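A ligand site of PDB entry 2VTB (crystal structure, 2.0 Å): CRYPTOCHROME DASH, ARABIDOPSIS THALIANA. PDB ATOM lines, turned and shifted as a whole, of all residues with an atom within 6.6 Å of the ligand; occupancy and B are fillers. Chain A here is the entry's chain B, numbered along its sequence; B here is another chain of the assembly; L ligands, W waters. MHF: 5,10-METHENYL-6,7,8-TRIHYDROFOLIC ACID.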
ATOM      1  N   THR A  83     -21.535 -13.175   1.621  1.00  0.00           N
ATOM      2  CA  THR A  83     -21.653 -12.888   0.193  1.00  0.00           C
ATOM      3  C   THR A  83     -20.508 -11.982  -0.274  1.00  0.00           C
ATOM      4  O   THR A  83     -19.857 -11.321   0.542  1.00  0.00           O
ATOM      5  CB  THR A  83     -23.013 -12.265  -0.159  1.00  0.00           C
ATOM      6  OG1 THR A  83     -23.220 -11.067   0.617  1.00  0.00           O
ATOM      7  CG2 THR A  83     -24.157 -13.255   0.116  1.00  0.00           C
ATOM      8  N   HIS A  84     -20.294 -11.949  -1.584  1.00  0.00           N
ATOM      9  CA  HIS A  84     -19.061 -11.412  -2.170  1.00  0.00           C
ATOM     10  C   HIS A  84     -18.848  -9.919  -1.929  1.00  0.00           C
ATOM     11  O   HIS A  84     -17.864  -9.528  -1.291  1.00  0.00           O
ATOM     12  CB  HIS A  84     -19.029 -11.719  -3.678  1.00  0.00           C
ATOM     13  CG  HIS A  84     -17.710 -11.429  -4.331  1.00  0.00           C
ATOM     14  ND1 HIS A  84     -16.739 -12.388  -4.501  1.00  0.00           N
ATOM     15  CD2 HIS A  84     -17.220 -10.287  -4.877  1.00  0.00           C
ATOM     16  CE1 HIS A  84     -15.700 -11.848  -5.118  1.00  0.00           C
ATOM     17  NE2 HIS A  84     -15.963 -10.577  -5.363  1.00  0.00           N
ATOM     18  N   PHE A  85     -19.751  -9.085  -2.432  1.00  0.00           N
ATOM     19  CA  PHE A  85     -19.580  -7.624  -2.380  1.00  0.00           C
ATOM     20  C   PHE A  85     -20.168  -6.989  -1.111  1.00  0.00           C
ATOM     21  O   PHE A  85     -19.558  -6.083  -0.560  1.00  0.00           O
ATOM     22  CB  PHE A  85     -20.176  -6.946  -3.626  1.00  0.00           C
ATOM     23  CG  PHE A  85     -19.514  -7.361  -4.916  1.00  0.00           C
ATOM     24  CD1 PHE A  85     -18.293  -6.812  -5.306  1.00  0.00           C
ATOM     25  CD2 PHE A  85     -20.112  -8.310  -5.758  1.00  0.00           C
ATOM     26  CE1 PHE A  85     -17.675  -7.199  -6.485  1.00  0.00           C
ATOM     27  CE2 PHE A  85     -19.499  -8.705  -6.947  1.00  0.00           C
ATOM     28  CZ  PHE A  85     -18.279  -8.145  -7.315  1.00  0.00           C
ATOM     29  N   LYS A  90     -23.724 -16.048   3.595  1.00  0.00           N
ATOM     30  CA  LYS A  90     -23.562 -16.797   2.350  1.00  0.00           C
ATOM     31  C   LYS A  90     -24.708 -17.796   2.178  1.00  0.00           C
ATOM     32  O   LYS A  90     -25.168 -18.031   1.068  1.00  0.00           O
ATOM     33  CB  LYS A  90     -22.201 -17.498   2.318  1.00  0.00           C
ATOM     34  CG  LYS A  90     -21.906 -18.306   1.037  1.00  0.00           C
ATOM     35  CD  LYS A  90     -21.762 -17.429  -0.193  1.00  0.00           C
ATOM     36  CE  LYS A  90     -21.275 -18.239  -1.402  1.00  0.00           C
ATOM     37  NZ  LYS A  90     -21.183 -17.426  -2.639  1.00  0.00           N
ATOM     38  N   CYS A 147     -19.502 -22.278 -12.243  1.00  0.00           N
ATOM     39  CA  CYS A 147     -19.110 -20.951 -11.729  1.00  0.00           C
ATOM     40  C   CYS A 147     -17.782 -20.942 -10.958  1.00  0.00           C
ATOM     41  O   CYS A 147     -17.332 -21.964 -10.453  1.00  0.00           O
ATOM     42  CB  CYS A 147     -20.237 -20.333 -10.887  1.00  0.00           C
ATOM     43  SG  CYS A 147     -21.727 -19.944 -11.871  1.00  0.00           S
ATOM     44  N   SER A 148     -17.175 -19.758 -10.888  1.00  0.00           N
ATOM     45  CA  SER A 148     -15.838 -19.528 -10.299  1.00  0.00           C
ATOM     46  C   SER A 148     -15.561 -20.292  -9.002  1.00  0.00           C
ATOM     47  O   SER A 148     -14.552 -20.989  -8.899  1.00  0.00           O
ATOM     48  CB  SER A 148     -15.604 -18.023 -10.091  1.00  0.00           C
ATOM     49  OG  SER A 148     -14.561 -17.754  -9.159  1.00  0.00           O
ATOM     50  N   GLU A 149     -16.433 -20.136  -8.010  1.00  0.00           N
ATOM     51  CA  GLU A 149     -16.182 -20.702  -6.679  1.00  0.00           C
ATOM     52  C   GLU A 149     -16.147 -22.225  -6.728  1.00  0.00           C
ATOM     53  O   GLU A 149     -15.254 -22.848  -6.142  1.00  0.00           O
ATOM     54  CB  GLU A 149     -17.232 -20.212  -5.668  1.00  0.00           C
ATOM     55  CG  GLU A 149     -17.020 -18.745  -5.256  1.00  0.00           C
ATOM     56  CD  GLU A 149     -18.184 -18.164  -4.462  1.00  0.00           C
ATOM     57  OE1 GLU A 149     -19.112 -18.925  -4.077  1.00  0.00           O
ATOM     58  OE2 GLU A 149     -18.174 -16.942  -4.226  1.00  0.00           O
ATOM     59  N   GLU A 150     -17.085 -22.822  -7.453  1.00  0.00           N
ATOM     60  CA  GLU A 150     -17.215 -24.268  -7.551  1.00  0.00           C
ATOM     61  C   GLU A 150     -16.062 -24.865  -8.364  1.00  0.00           C
ATOM     62  O   GLU A 150     -15.492 -25.885  -7.990  1.00  0.00           O
ATOM     63  CB  GLU A 150     -18.559 -24.670  -8.175  1.00  0.00           C
ATOM     64  CG  GLU A 150     -19.772 -24.499  -7.250  1.00  0.00           C
ATOM     65  CD  GLU A 150     -20.047 -23.049  -6.897  1.00  0.00           C
ATOM     66  OE1 GLU A 150     -20.114 -22.204  -7.822  1.00  0.00           O
ATOM     67  OE2 GLU A 150     -20.185 -22.752  -5.678  1.00  0.00           O
ATOM     68  N   ASN A 342     -17.047 -14.695 -15.110  1.00  0.00           N
ATOM     69  CA  ASN A 342     -17.272 -13.794 -13.974  1.00  0.00           C
ATOM     70  C   ASN A 342     -17.966 -12.465 -14.330  1.00  0.00           C
ATOM     71  O   ASN A 342     -18.382 -11.734 -13.424  1.00  0.00           O
ATOM     72  CB  ASN A 342     -15.952 -13.537 -13.248  1.00  0.00           C
ATOM     73  CG  ASN A 342     -15.403 -14.796 -12.599  1.00  0.00           C
ATOM     74  OD1 ASN A 342     -16.142 -15.708 -12.267  1.00  0.00           O
ATOM     75  ND2 ASN A 342     -14.082 -14.845 -12.411  1.00  0.00           N
ATOM     76  N   SER A 343     -18.104 -12.182 -15.623  1.00  0.00           N
ATOM     77  CA  SER A 343     -18.856 -11.012 -16.076  1.00  0.00           C
ATOM     78  C   SER A 343     -20.343 -11.099 -15.663  1.00  0.00           C
ATOM     79  O   SER A 343     -21.027 -10.081 -15.592  1.00  0.00           O
ATOM     80  CB  SER A 343     -18.725 -10.826 -17.593  1.00  0.00           C
ATOM     81  OG  SER A 343     -19.482 -11.792 -18.300  1.00  0.00           O
ATOM     82  N   PHE A 345     -21.224 -11.635 -12.732  1.00  0.00           N
ATOM     83  CA  PHE A 345     -21.276 -11.083 -11.381  1.00  0.00           C
ATOM     84  C   PHE A 345     -20.849  -9.619 -11.287  1.00  0.00           C
ATOM     85  O   PHE A 345     -20.937  -9.000 -10.219  1.00  0.00           O
ATOM     86  CB  PHE A 345     -20.369 -11.918 -10.462  1.00  0.00           C
ATOM     87  CG  PHE A 345     -20.653 -13.382 -10.507  1.00  0.00           C
ATOM     88  CD1 PHE A 345     -21.901 -13.874 -10.158  1.00  0.00           C
ATOM     89  CD2 PHE A 345     -19.671 -14.286 -10.917  1.00  0.00           C
ATOM     90  CE1 PHE A 345     -22.161 -15.240 -10.197  1.00  0.00           C
ATOM     91  CE2 PHE A 345     -19.928 -15.641 -10.966  1.00  0.00           C
ATOM     92  CZ  PHE A 345     -21.180 -16.121 -10.605  1.00  0.00           C
ATOM     93  N   HIS A 346     -20.384  -9.046 -12.402  1.00  0.00           N
ATOM     94  CA  HIS A 346     -19.872  -7.696 -12.403  1.00  0.00           C
ATOM     95  C   HIS A 346     -20.994  -6.680 -12.621  1.00  0.00           C
ATOM     96  O   HIS A 346     -21.995  -6.987 -13.258  1.00  0.00           O
ATOM     97  CB  HIS A 346     -18.778  -7.535 -13.451  1.00  0.00           C
ATOM     98  CG  HIS A 346     -17.562  -8.363 -13.188  1.00  0.00           C
ATOM     99  ND1 HIS A 346     -16.659  -8.721 -14.175  1.00  0.00           N
ATOM    100  CD2 HIS A 346     -17.098  -8.924 -12.033  1.00  0.00           C
ATOM    101  CE1 HIS A 346     -15.697  -9.440 -13.639  1.00  0.00           C
ATOM    102  NE2 HIS A 346     -15.931  -9.584 -12.346  1.00  0.00           N
ATOM    103  N   GLU A 415     -27.506 -10.367  -4.225  1.00  0.00           N
ATOM    104  CA  GLU A 415     -26.887 -10.988  -3.048  1.00  0.00           C
ATOM    105  C   GLU A 415     -27.893 -11.280  -1.935  1.00  0.00           C
ATOM    106  O   GLU A 415     -27.753 -12.265  -1.217  1.00  0.00           O
ATOM    107  CB  GLU A 415     -25.708 -10.166  -2.531  1.00  0.00           C
ATOM    108  CG  GLU A 415     -24.474 -10.326  -3.428  1.00  0.00           C
ATOM    109  CD  GLU A 415     -23.195  -9.761  -2.829  1.00  0.00           C
ATOM    110  OE1 GLU A 415     -23.190  -9.352  -1.653  1.00  0.00           O
ATOM    111  OE2 GLU A 415     -22.177  -9.760  -3.555  1.00  0.00           O
ATOM    112  N   GLU A 418     -29.459 -14.367  -2.932  1.00  0.00           N
ATOM    113  CA  GLU A 418     -28.505 -15.449  -2.674  1.00  0.00           C
ATOM    114  C   GLU A 418     -28.556 -15.924  -1.218  1.00  0.00           C
ATOM    115  O   GLU A 418     -28.434 -17.120  -0.954  1.00  0.00           O
ATOM    116  CB  GLU A 418     -27.072 -15.053  -3.051  1.00  0.00           C
ATOM    117  CG  GLU A 418     -26.013 -16.068  -2.589  1.00  0.00           C
ATOM    118  CD  GLU A 418     -24.647 -15.898  -3.241  1.00  0.00           C
ATOM    119  OE1 GLU A 418     -24.406 -14.859  -3.900  1.00  0.00           O
ATOM    120  OE2 GLU A 418     -23.804 -16.817  -3.072  1.00  0.00           O
ATOM    121  N   TYR A 424     -31.709 -20.965  -4.566  1.00  0.00           N
ATOM    122  CA  TYR A 424     -30.590 -20.179  -5.060  1.00  0.00           C
ATOM    123  C   TYR A 424     -29.668 -21.033  -5.944  1.00  0.00           C
ATOM    124  O   TYR A 424     -29.238 -22.119  -5.564  1.00  0.00           O
ATOM    125  CB  TYR A 424     -29.744 -19.572  -3.923  1.00  0.00           C
ATOM    126  CG  TYR A 424     -28.462 -19.013  -4.484  1.00  0.00           C
ATOM    127  CD1 TYR A 424     -28.482 -17.905  -5.330  1.00  0.00           C
ATOM    128  CD2 TYR A 424     -27.226 -19.620  -4.234  1.00  0.00           C
ATOM    129  CE1 TYR A 424     -27.323 -17.400  -5.878  1.00  0.00           C
ATOM    130  CE2 TYR A 424     -26.058 -19.119  -4.783  1.00  0.00           C
ATOM    131  CZ  TYR A 424     -26.116 -18.005  -5.603  1.00  0.00           C
ATOM    132  OH  TYR A 424     -24.978 -17.468  -6.164  1.00  0.00           O
ATOM    133  N   ASP A 425     -29.384 -20.485  -7.124  1.00  0.00           N
ATOM    134  CA  ASP A 425     -28.507 -21.094  -8.120  1.00  0.00           C
ATOM    135  C   ASP A 425     -27.779 -19.927  -8.761  1.00  0.00           C
ATOM    136  O   ASP A 425     -28.435 -18.987  -9.211  1.00  0.00           O
ATOM    137  CB  ASP A 425     -29.391 -21.830  -9.152  1.00  0.00           C
ATOM    138  CG  ASP A 425     -28.599 -22.407 -10.314  1.00  0.00           C
ATOM    139  OD1 ASP A 425     -28.766 -23.623 -10.567  1.00  0.00           O
ATOM    140  OD2 ASP A 425     -27.853 -21.655 -10.978  1.00  0.00           O
ATOM    141  N   PRO A 426     -26.429 -19.963  -8.790  1.00  0.00           N
ATOM    142  CA  PRO A 426     -25.737 -18.760  -9.300  1.00  0.00           C
ATOM    143  C   PRO A 426     -26.073 -18.449 -10.754  1.00  0.00           C
ATOM    144  O   PRO A 426     -26.227 -17.280 -11.117  1.00  0.00           O
ATOM    145  CB  PRO A 426     -24.249 -19.117  -9.137  1.00  0.00           C
ATOM    146  CG  PRO A 426     -24.210 -20.589  -9.110  1.00  0.00           C
ATOM    147  CD  PRO A 426     -25.468 -21.007  -8.418  1.00  0.00           C
ATOM    148  N   TYR A 430     -28.079 -14.871 -10.947  1.00  0.00           N
ATOM    149  CA  TYR A 430     -27.349 -13.760 -11.564  1.00  0.00           C
ATOM    150  C   TYR A 430     -27.692 -13.621 -13.053  1.00  0.00           C
ATOM    151  O   TYR A 430     -27.685 -12.510 -13.598  1.00  0.00           O
ATOM    152  CB  TYR A 430     -25.837 -13.867 -11.289  1.00  0.00           C
ATOM    153  CG  TYR A 430     -25.493 -13.598  -9.822  1.00  0.00           C
ATOM    154  CD1 TYR A 430     -25.211 -12.307  -9.387  1.00  0.00           C
ATOM    155  CD2 TYR A 430     -25.476 -14.631  -8.887  1.00  0.00           C
ATOM    156  CE1 TYR A 430     -24.897 -12.055  -8.039  1.00  0.00           C
ATOM    157  CE2 TYR A 430     -25.177 -14.382  -7.547  1.00  0.00           C
ATOM    158  CZ  TYR A 430     -24.895 -13.102  -7.144  1.00  0.00           C
ATOM    159  OH  TYR A 430     -24.594 -12.865  -5.826  1.00  0.00           O
ATOM    160  N   PHE B 189     -10.860 -19.081 -15.394  1.00  0.00           N
ATOM    161  CA  PHE B 189     -11.914 -18.072 -15.257  1.00  0.00           C
ATOM    162  C   PHE B 189     -11.493 -16.946 -14.300  1.00  0.00           C
ATOM    163  O   PHE B 189     -11.993 -15.833 -14.422  1.00  0.00           O
ATOM    164  CB  PHE B 189     -13.232 -18.700 -14.779  1.00  0.00           C
ATOM    165  CG  PHE B 189     -14.110 -19.216 -15.892  1.00  0.00           C
ATOM    166  CD1 PHE B 189     -13.579 -19.573 -17.125  1.00  0.00           C
ATOM    167  CD2 PHE B 189     -15.476 -19.364 -15.685  1.00  0.00           C
ATOM    168  CE1 PHE B 189     -14.405 -20.038 -18.150  1.00  0.00           C
ATOM    169  CE2 PHE B 189     -16.307 -19.838 -16.710  1.00  0.00           C
ATOM    170  CZ  PHE B 189     -15.774 -20.174 -17.932  1.00  0.00           C
ATOM    171  N   ASP B 190     -10.590 -17.250 -13.381  1.00  0.00           N
ATOM    172  CA  ASP B 190     -10.051 -16.244 -12.454  1.00  0.00           C
ATOM    173  C   ASP B 190      -8.600 -15.857 -12.783  1.00  0.00           C
ATOM    174  O   ASP B 190      -7.855 -15.406 -11.910  1.00  0.00           O
ATOM    175  CB  ASP B 190     -10.190 -16.733 -11.015  1.00  0.00           C
ATOM    176  CG  ASP B 190     -11.586 -16.523 -10.486  1.00  0.00           C
ATOM    177  OD1 ASP B 190     -11.886 -15.406  -9.998  1.00  0.00           O
ATOM    178  OD2 ASP B 190     -12.389 -17.439 -10.581  1.00  0.00           O
ATOM    179  N   LEU B 191      -8.221 -16.022 -14.046  1.00  0.00           N
ATOM    180  CA  LEU B 191      -6.902 -15.592 -14.513  1.00  0.00           C
ATOM    181  C   LEU B 191      -6.760 -14.101 -14.230  1.00  0.00           C
ATOM    182  O   LEU B 191      -7.663 -13.327 -14.536  1.00  0.00           O
ATOM    183  CB  LEU B 191      -6.764 -15.861 -16.023  1.00  0.00           C
ATOM    184  CG  LEU B 191      -5.365 -15.707 -16.641  1.00  0.00           C
ATOM    185  CD1 LEU B 191      -4.498 -16.907 -16.269  1.00  0.00           C
ATOM    186  CD2 LEU B 191      -5.467 -15.546 -18.145  1.00  0.00           C
ATOM    187  N   PRO B 192      -5.637 -13.686 -13.622  1.00  0.00           N
ATOM    188  CA  PRO B 192      -5.441 -12.250 -13.445  1.00  0.00           C
ATOM    189  C   PRO B 192      -5.506 -11.472 -14.773  1.00  0.00           C
ATOM    190  O   PRO B 192      -4.977 -11.933 -15.783  1.00  0.00           O
ATOM    191  CB  PRO B 192      -4.039 -12.160 -12.829  1.00  0.00           C
ATOM    192  CG  PRO B 192      -3.850 -13.464 -12.149  1.00  0.00           C
ATOM    193  CD  PRO B 192      -4.524 -14.464 -13.034  1.00  0.00           C
ATOM    194  N   ASP B 193      -6.168 -10.310 -14.753  1.00  0.00           N
ATOM    195  CA  ASP B 193      -6.222  -9.431 -15.922  1.00  0.00           C
ATOM    196  C   ASP B 193      -4.924  -8.646 -16.128  1.00  0.00           C
ATOM    197  O   ASP B 193      -4.796  -7.954 -17.129  1.00  0.00           O
ATOM    198  CB  ASP B 193      -7.409  -8.448 -15.828  1.00  0.00           C
ATOM    199  CG  ASP B 193      -8.743  -9.069 -16.241  1.00  0.00           C
ATOM    200  OD1 ASP B 193      -8.769 -10.177 -16.820  1.00  0.00           O
ATOM    201  OD2 ASP B 193      -9.768  -8.418 -15.980  1.00  0.00           O
ATOM    202  N   GLN B 197       0.822  -9.977 -12.445  1.00  0.00           N
ATOM    203  CA  GLN B 197       0.183 -10.723 -11.371  1.00  0.00           C
ATOM    204  C   GLN B 197       0.150 -12.230 -11.682  1.00  0.00           C
ATOM    205  O   GLN B 197       0.415 -13.055 -10.816  1.00  0.00           O
ATOM    206  CB  GLN B 197      -1.215 -10.143 -11.080  1.00  0.00           C
ATOM    207  CG  GLN B 197      -1.165  -8.681 -10.572  1.00  0.00           C
ATOM    208  CD  GLN B 197      -2.535  -8.011 -10.460  1.00  0.00           C
ATOM    209  OE1 GLN B 197      -3.560  -8.677 -10.335  1.00  0.00           O
ATOM    210  NE2 GLN B 197      -2.549  -6.672 -10.503  1.00  0.00           N
ATOM    211  N   LYS B 339     -10.445 -17.419 -20.909  1.00  0.00           N
ATOM    212  CA  LYS B 339     -11.180 -16.475 -20.076  1.00  0.00           C
ATOM    213  C   LYS B 339     -12.052 -15.547 -20.921  1.00  0.00           C
ATOM    214  O   LYS B 339     -13.219 -15.317 -20.577  1.00  0.00           O
ATOM    215  CB  LYS B 339     -10.237 -15.642 -19.197  1.00  0.00           C
ATOM    216  CG  LYS B 339     -10.977 -14.720 -18.223  1.00  0.00           C
ATOM    217  CD  LYS B 339     -10.042 -14.018 -17.253  1.00  0.00           C
ATOM    218  CE  LYS B 339     -10.797 -13.021 -16.361  1.00  0.00           C
ATOM    219  NZ  LYS B 339      -9.904 -12.220 -15.488  1.00  0.00           N
HETATM  220  N1  MHF L   1     -22.229 -18.164  -5.902  1.00  0.00           N
HETATM  221  C2  MHF L   1     -21.747 -19.344  -6.343  1.00  0.00           C
HETATM  222  NA2 MHF L   1     -22.399 -20.462  -5.993  1.00  0.00           N
HETATM  223  N3  MHF L   1     -20.617 -19.448  -7.106  1.00  0.00           N
HETATM  224  C4  MHF L   1     -19.902 -18.369  -7.490  1.00  0.00           C
HETATM  225  O4  MHF L   1     -18.877 -18.492  -8.178  1.00  0.00           O
HETATM  226  C4A MHF L   1     -20.382 -17.048  -7.026  1.00  0.00           C
HETATM  227  N5  MHF L   1     -19.812 -15.805  -7.341  1.00  0.00           N
HETATM  228  C6  MHF L   1     -19.995 -14.789  -6.311  1.00  0.00           C
HETATM  229  C7  MHF L   1     -21.487 -14.547  -6.170  1.00  0.00           C
HETATM  230  N8  MHF L   1     -22.102 -15.815  -5.800  1.00  0.00           N
HETATM  231  C8A MHF L   1     -21.610 -17.010  -6.213  1.00  0.00           C
HETATM  232  C9  MHF L   1     -19.164 -13.616  -6.836  1.00  0.00           C
HETATM  233  N10 MHF L   1     -18.410 -14.222  -7.955  1.00  0.00           N
HETATM  234  C11 MHF L   1     -18.406 -15.682  -7.739  1.00  0.00           C
HETATM  235  C12 MHF L   1     -14.926 -12.404  -9.528  1.00  0.00           C
HETATM  236  C13 MHF L   1     -15.005 -13.791  -9.394  1.00  0.00           C
HETATM  237  C14 MHF L   1     -16.146 -14.392  -8.869  1.00  0.00           C
HETATM  238  C15 MHF L   1     -17.223 -13.610  -8.435  1.00  0.00           C
HETATM  239  C16 MHF L   1     -17.161 -12.226  -8.597  1.00  0.00           C
HETATM  240  C17 MHF L   1     -16.027 -11.633  -9.132  1.00  0.00           C
HETATM  241  C   MHF L   1     -13.709 -11.748 -10.131  1.00  0.00           C
HETATM  242  O   MHF L   1     -13.842 -10.610 -10.540  1.00  0.00           O
HETATM  243  N   MHF L   1     -12.548 -12.409 -10.301  1.00  0.00           N
HETATM  244  CA  MHF L   1     -11.420 -11.820 -11.029  1.00  0.00           C
HETATM  245  CB  MHF L   1     -10.125 -12.587 -10.732  1.00  0.00           C
HETATM  246  CG  MHF L   1      -9.775 -12.608  -9.254  1.00  0.00           C
HETATM  247  CD  MHF L   1      -9.712 -11.208  -8.703  1.00  0.00           C
HETATM  248  OE1 MHF L   1     -10.473 -10.937  -7.757  1.00  0.00           O
HETATM  249  OE2 MHF L   1      -8.915 -10.384  -9.225  1.00  0.00           O
HETATM  250  CT  MHF L   1     -11.591 -11.793 -12.524  1.00  0.00           C
HETATM  251  O1  MHF L   1     -10.826 -11.049 -13.191  1.00  0.00           O
HETATM  252  O2  MHF L   1     -12.470 -12.510 -13.067  1.00  0.00           O
HETATM  253  O   HOH W   1     -21.897 -13.729  -3.122  1.00  0.00           O
HETATM  254  O   HOH W   2     -22.119 -11.388  -6.016  1.00  0.00           O
HETATM  255  O   HOH W   3      -8.136  -9.963 -12.689  1.00  0.00           O
HETATM  256  O   HOH W   4     -13.564 -11.272 -15.240  1.00  0.00           O
HETATM  257  O   HOH W   5     -20.198 -21.115  -3.518  1.00  0.00           O
HETATM  258  O   HOH W   6     -23.340 -21.017  -2.984  1.00  0.00           O
HETATM  259  O   HOH W   7      -6.943 -14.561  -9.571  1.00  0.00           O
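O of Leu 191 of chain B lies within hydrogen-bond range of NZ of Lys 339 of chain B (2.7 Å). The backbone NH (N) of His 84 lies within hydrogen-bond range of the side-chain carboxylate (OE2) of Glu 415. O of Asn 342 sits close to NE2 of His 346, 3.4 Å away. NZ of Lys 339 of chain B is in salt-bridge range of OD1 of Asp 193 of chain B, 2.7 Å away. NZ of Lys 90 lies within salt-bridge range of OE1 of Glu 149 (2.9 Å). The side-chain amide nitrogen (ND2) of Asn 342 sits at hydrogen-bond distance from the backbone carbonyl oxygen (O) of Phe 189 of chain B, at 3.1 Å. The side-chain carboxylate (OE2) of Glu 418 is in salt-bridge range of the side-chain amino group (NZ) of Lys 90 (2.7 Å). The side-chain hydroxyl of Tyr 424 lies close to the side-chain carboxylate of Glu 418 (3.4 Å).
The side-chain carboxylate (OE1) of Glu 418 is in hydrogen-bond range of a nitrogen (N8) of the ligand, at 3.1 Å. A ring nitrogen (NE2) of His 346 sits at hydrogen-bond distance from an oxygen (O) of the ligand (2.9 Å). An oxygen (O1) of the ligand lies within salt-bridge range of the side-chain amino group (NZ) of Lys 339 of chain B. OE1 of Glu 150 sits at hydrogen-bond distance from N3 of the ligand. ND2 of Asn 342 lies within hydrogen-bond range of O2 of the ligand, at 2.9 Å. N1 of the ligand sits at hydrogen-bond distance from OH of Tyr 424 (2.8 Å). OD1 of Asp 190 of chain B lies within hydrogen-bond range of N of the ligand, at 3.1 Å. The backbone NH (N) of Glu 149 sits at hydrogen-bond distance from an oxygen (O4) of the ligand (3.0 Å). N of Ser 148 is in hydrogen-bond range of O4 of the ligand (3.4 Å). A nitrogen (N3) of the ligand lies close to the side-chain carboxylate (OE1) of Glu 149 (3.4 Å).
Water W3 lies within hydrogen-bond range of the backbone NH (N) of Asp 193 of chain B (2.9 Å) and an oxygen (O1) of the ligand (2.9 Å). Water W1 lies within hydrogen-bond range of N of His 84, OE1 of Glu 418 and N8 of the ligand. Water W2 lies within hydrogen-bond range of the side-chain hydroxyl (OH) of Tyr 430 (2.9 Å) and the side-chain carboxylate (OE2) of Glu 415 (3.0 Å). Water W5 lies within hydrogen-bond range of the side-chain carboxylate of Glu 149, the side-chain carboxylate of Glu 150 and a nitrogen (NA2) of the ligand.
Residues that only touch the ligand: His 84 (3.6 Å), Lys 90 (3.5 Å), Cys 147 (3.5 Å), Phe 345 (3.2 Å), Pro 426 (3.6 Å), Tyr 430 (3.5 Å), Phe 189 of chain B (3.6 Å) and Asp 193 of chain B (3.98 Å). 17 residues have an atom within 4 Å of the ligand: His 84, Lys 90, Cys 147, Ser 148, Glu 149, Glu 150, Asn 342, Phe 345, His 346, Glu 418, Tyr 424, Pro 426, Tyr 430, Phe 189 of chain B, Asp 190 of chain B, Asp 193 of chain B and Lys 339 of chain B.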
